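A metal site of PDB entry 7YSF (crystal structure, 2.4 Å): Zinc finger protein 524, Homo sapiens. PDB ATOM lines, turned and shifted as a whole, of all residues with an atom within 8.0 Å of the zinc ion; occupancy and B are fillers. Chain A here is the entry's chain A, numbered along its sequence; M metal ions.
O of Arg 73 is in hydrogen-bond range of N of Cys 68 (3.1 Å).
SG of Cys 71 sits close to N of Arg 73, at 3.5 Å.
The side-chain sulfur (SG) of Cys 68 sits close to the backbone NH (N) of Leu 70 (3.5 Å).
The zinc ion is bound by a ring nitrogen (NE2) of His 88 (2.1 Å), a ring nitrogen (NE2) of His 84 (2.1 Å), the side-chain sulfur of Cys 68 (2.2 Å) and the side-chain sulfur of Cys 71 (2.3 Å).
Four residues have an atom within 4 Å of the zinc ion: Cys 68, Cys 71, His 84 and His 88.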
ATOM      1  N   ARG A  67      17.453  12.065 -15.586  1.00  0.00           N
ATOM      2  CA  ARG A  67      17.753  10.689 -15.223  1.00  0.00           C
ATOM      3  C   ARG A  67      19.164  10.306 -15.627  1.00  0.00           C
ATOM      4  O   ARG A  67      19.627  10.623 -16.725  1.00  0.00           O
ATOM      5  CB  ARG A  67      16.759   9.731 -15.901  1.00  0.00           C
ATOM      6  CG  ARG A  67      15.317   9.962 -15.568  1.00  0.00           C
ATOM      7  CD  ARG A  67      14.506   8.725 -15.876  1.00  0.00           C
ATOM      8  NE  ARG A  67      13.428   8.988 -16.822  1.00  0.00           N
ATOM      9  CZ  ARG A  67      12.540   8.085 -17.215  1.00  0.00           C
ATOM     10  NH1 ARG A  67      12.602   6.849 -16.741  1.00  0.00           N
ATOM     11  NH2 ARG A  67      11.593   8.412 -18.074  1.00  0.00           N
ATOM     12  N   CYS A  68      19.842   9.597 -14.739  1.00  0.00           N
ATOM     13  CA  CYS A  68      21.140   9.014 -15.078  1.00  0.00           C
ATOM     14  C   CYS A  68      20.929   7.754 -15.902  1.00  0.00           C
ATOM     15  O   CYS A  68      20.178   6.870 -15.474  1.00  0.00           O
ATOM     16  CB  CYS A  68      21.928   8.694 -13.814  1.00  0.00           C
ATOM     17  SG  CYS A  68      23.550   7.978 -14.142  1.00  0.00           S
ATOM     18  N   PRO A  69      21.543   7.627 -17.075  1.00  0.00           N
ATOM     19  CA  PRO A  69      21.366   6.407 -17.871  1.00  0.00           C
ATOM     20  C   PRO A  69      21.923   5.162 -17.208  1.00  0.00           C
ATOM     21  O   PRO A  69      21.540   4.048 -17.580  1.00  0.00           O
ATOM     22  CB  PRO A  69      22.092   6.718 -19.191  1.00  0.00           C
ATOM     23  CG  PRO A  69      22.163   8.202 -19.234  1.00  0.00           C
ATOM     24  CD  PRO A  69      22.275   8.674 -17.823  1.00  0.00           C
ATOM     25  N   LEU A  70      22.815   5.310 -16.220  1.00  0.00           N
ATOM     26  CA  LEU A  70      23.549   4.188 -15.652  1.00  0.00           C
ATOM     27  C   LEU A  70      23.039   3.739 -14.297  1.00  0.00           C
ATOM     28  O   LEU A  70      23.456   2.673 -13.823  1.00  0.00           O
ATOM     29  CB  LEU A  70      25.040   4.551 -15.550  1.00  0.00           C
ATOM     30  CG  LEU A  70      25.636   5.123 -16.842  1.00  0.00           C
ATOM     31  CD1 LEU A  70      27.096   5.487 -16.665  1.00  0.00           C
ATOM     32  CD2 LEU A  70      25.454   4.138 -17.993  1.00  0.00           C
ATOM     33  N   CYS A  71      22.171   4.509 -13.654  1.00  0.00           N
ATOM     34  CA  CYS A  71      21.636   4.151 -12.345  1.00  0.00           C
ATOM     35  C   CYS A  71      20.286   4.825 -12.189  1.00  0.00           C
ATOM     36  O   CYS A  71      19.901   5.667 -13.015  1.00  0.00           O
ATOM     37  CB  CYS A  71      22.609   4.555 -11.214  1.00  0.00           C
ATOM     38  SG  CYS A  71      22.624   6.300 -10.825  1.00  0.00           S
ATOM     39  N   PRO A  72      19.516   4.473 -11.151  1.00  0.00           N
ATOM     40  CA  PRO A  72      18.172   5.055 -10.975  1.00  0.00           C
ATOM     41  C   PRO A  72      18.148   6.448 -10.365  1.00  0.00           C
ATOM     42  O   PRO A  72      17.059   6.929 -10.039  1.00  0.00           O
ATOM     43  CB  PRO A  72      17.478   4.044 -10.039  1.00  0.00           C
ATOM     44  CG  PRO A  72      18.374   2.847  -9.965  1.00  0.00           C
ATOM     45  CD  PRO A  72      19.740   3.373 -10.196  1.00  0.00           C
ATOM     46  N   ARG A  73      19.280   7.122 -10.208  1.00  0.00           N
ATOM     47  CA  ARG A  73      19.286   8.426  -9.570  1.00  0.00           C
ATOM     48  C   ARG A  73      18.852   9.522 -10.531  1.00  0.00           C
ATOM     49  O   ARG A  73      19.143   9.464 -11.738  1.00  0.00           O
ATOM     50  CB  ARG A  73      20.669   8.743  -8.988  1.00  0.00           C
ATOM     51  CG  ARG A  73      20.717   8.734  -7.465  1.00  0.00           C
ATOM     52  CD  ARG A  73      22.139   8.850  -6.944  1.00  0.00           C
ATOM     53  NE  ARG A  73      22.874   7.595  -7.058  1.00  0.00           N
ATOM     54  CZ  ARG A  73      22.839   6.629  -6.141  1.00  0.00           C
ATOM     55  NH1 ARG A  73      22.097   6.756  -5.050  1.00  0.00           N
ATOM     56  NH2 ARG A  73      23.547   5.514  -6.323  1.00  0.00           N
ATOM     57  N   ARG A  74      18.154  10.515  -9.999  1.00  0.00           N
ATOM     58  CA  ARG A  74      17.643  11.640 -10.777  1.00  0.00           C
ATOM     59  C   ARG A  74      18.131  12.946 -10.172  1.00  0.00           C
ATOM     60  O   ARG A  74      18.538  13.010  -9.009  1.00  0.00           O
ATOM     61  CB  ARG A  74      16.109  11.642 -10.827  1.00  0.00           C
ATOM     62  CG  ARG A  74      15.494  10.407 -11.440  1.00  0.00           C
ATOM     63  CD  ARG A  74      13.993  10.413 -11.228  1.00  0.00           C
ATOM     64  NE  ARG A  74      13.312   9.358 -11.956  1.00  0.00           N
ATOM     65  CZ  ARG A  74      12.714   9.542 -13.127  1.00  0.00           C
ATOM     66  NH1 ARG A  74      12.103   8.528 -13.736  1.00  0.00           N
ATOM     67  NH2 ARG A  74      12.713  10.738 -13.698  1.00  0.00           N
ATOM     68  N   PHE A  75      18.091  14.000 -10.981  1.00  0.00           N
ATOM     69  CA  PHE A  75      18.708  15.269 -10.603  1.00  0.00           C
ATOM     70  C   PHE A  75      17.900  16.439 -11.151  1.00  0.00           C
ATOM     71  O   PHE A  75      17.240  16.334 -12.190  1.00  0.00           O
ATOM     72  CB  PHE A  75      20.154  15.320 -11.095  1.00  0.00           C
ATOM     73  CG  PHE A  75      21.003  14.220 -10.553  1.00  0.00           C
ATOM     74  CD1 PHE A  75      21.612  14.349  -9.315  1.00  0.00           C
ATOM     75  CD2 PHE A  75      21.156  13.029 -11.245  1.00  0.00           C
ATOM     76  CE1 PHE A  75      22.381  13.340  -8.795  1.00  0.00           C
ATOM     77  CE2 PHE A  75      21.918  12.004 -10.722  1.00  0.00           C
ATOM     78  CZ  PHE A  75      22.531  12.156  -9.494  1.00  0.00           C
ATOM     79  N   LEU A  81      23.696  16.209 -12.896  1.00  0.00           N
ATOM     80  CA  LEU A  81      23.857  14.874 -13.442  1.00  0.00           C
ATOM     81  C   LEU A  81      25.267  14.672 -13.987  1.00  0.00           C
ATOM     82  O   LEU A  81      25.838  13.590 -13.866  1.00  0.00           O
ATOM     83  CB  LEU A  81      22.819  14.625 -14.549  1.00  0.00           C
ATOM     84  CG  LEU A  81      23.000  13.407 -15.448  1.00  0.00           C
ATOM     85  CD1 LEU A  81      23.062  12.127 -14.628  1.00  0.00           C
ATOM     86  CD2 LEU A  81      21.896  13.320 -16.493  1.00  0.00           C
ATOM     87  N   HIS A  84      27.440  13.983 -11.157  1.00  0.00           N
ATOM     88  CA  HIS A  84      27.163  12.629 -10.711  1.00  0.00           C
ATOM     89  C   HIS A  84      27.855  11.585 -11.580  1.00  0.00           C
ATOM     90  O   HIS A  84      28.215  10.513 -11.090  1.00  0.00           O
ATOM     91  CB  HIS A  84      25.656  12.369 -10.714  1.00  0.00           C
ATOM     92  CG  HIS A  84      25.303  10.920 -10.576  1.00  0.00           C
ATOM     93  ND1 HIS A  84      25.377  10.245  -9.370  1.00  0.00           N
ATOM     94  CD2 HIS A  84      24.867  10.012 -11.479  1.00  0.00           C
ATOM     95  CE1 HIS A  84      25.004   8.993  -9.545  1.00  0.00           C
ATOM     96  NE2 HIS A  84      24.692   8.829 -10.822  1.00  0.00           N
ATOM     97  N   HIS A  85      28.057  11.889 -12.868  1.00  0.00           N
ATOM     98  CA  HIS A  85      28.671  10.909 -13.759  1.00  0.00           C
ATOM     99  C   HIS A  85      30.083  10.549 -13.340  1.00  0.00           C
ATOM    100  O   HIS A  85      30.592   9.494 -13.753  1.00  0.00           O
ATOM    101  CB  HIS A  85      28.675  11.435 -15.199  1.00  0.00           C
ATOM    102  CG  HIS A  85      29.148  10.425 -16.197  1.00  0.00           C
ATOM    103  ND1 HIS A  85      28.311   9.483 -16.759  1.00  0.00           N
ATOM    104  CD2 HIS A  85      30.380  10.187 -16.721  1.00  0.00           C
ATOM    105  CE1 HIS A  85      28.997   8.730 -17.592  1.00  0.00           C
ATOM    106  NE2 HIS A  85      30.259   9.131 -17.580  1.00  0.00           N
ATOM    107  N   ARG A  86      30.735  11.377 -12.520  1.00  0.00           N
ATOM    108  CA  ARG A  86      32.059  11.012 -12.009  1.00  0.00           C
ATOM    109  C   ARG A  86      31.992   9.744 -11.154  1.00  0.00           C
ATOM    110  O   ARG A  86      32.968   8.998 -11.077  1.00  0.00           O
ATOM    111  CB  ARG A  86      32.652  12.169 -11.212  1.00  0.00           C
ATOM    112  CG  ARG A  86      33.440  13.146 -12.057  1.00  0.00           C
ATOM    113  CD  ARG A  86      33.501  14.520 -11.412  1.00  0.00           C
ATOM    114  NE  ARG A  86      33.858  15.548 -12.385  1.00  0.00           N
ATOM    115  CZ  ARG A  86      33.656  16.852 -12.216  1.00  0.00           C
ATOM    116  NH1 ARG A  86      33.102  17.300 -11.094  1.00  0.00           N
ATOM    117  NH2 ARG A  86      34.012  17.707 -13.157  1.00  0.00           N
ATOM    118  N   VAL A  87      30.845   9.498 -10.510  1.00  0.00           N
ATOM    119  CA  VAL A  87      30.658   8.254  -9.774  1.00  0.00           C
ATOM    120  C   VAL A  87      30.908   7.052 -10.685  1.00  0.00           C
ATOM    121  O   VAL A  87      31.507   6.053 -10.278  1.00  0.00           O
ATOM    122  CB  VAL A  87      29.245   8.219  -9.160  1.00  0.00           C
ATOM    123  CG1 VAL A  87      28.810   6.785  -8.866  1.00  0.00           C
ATOM    124  CG2 VAL A  87      29.193   9.074  -7.897  1.00  0.00           C
ATOM    125  N   HIS A  88      30.475   7.151 -11.938  1.00  0.00           N
ATOM    126  CA  HIS A  88      30.615   6.050 -12.892  1.00  0.00           C
ATOM    127  C   HIS A  88      31.940   6.107 -13.658  1.00  0.00           C
ATOM    128  O   HIS A  88      32.549   5.074 -13.893  1.00  0.00           O
ATOM    129  CB  HIS A  88      29.435   6.059 -13.866  1.00  0.00           C
ATOM    130  CG  HIS A  88      28.108   5.990 -13.187  1.00  0.00           C
ATOM    131  ND1 HIS A  88      27.731   4.922 -12.414  1.00  0.00           N
ATOM    132  CD2 HIS A  88      27.071   6.862 -13.166  1.00  0.00           C
ATOM    133  CE1 HIS A  88      26.511   5.120 -11.938  1.00  0.00           C
ATOM    134  NE2 HIS A  88      26.088   6.298 -12.382  1.00  0.00           N
HETATM  135 ZN    ZN M   1      24.269   7.242 -12.169  1.00  0.00          ZN
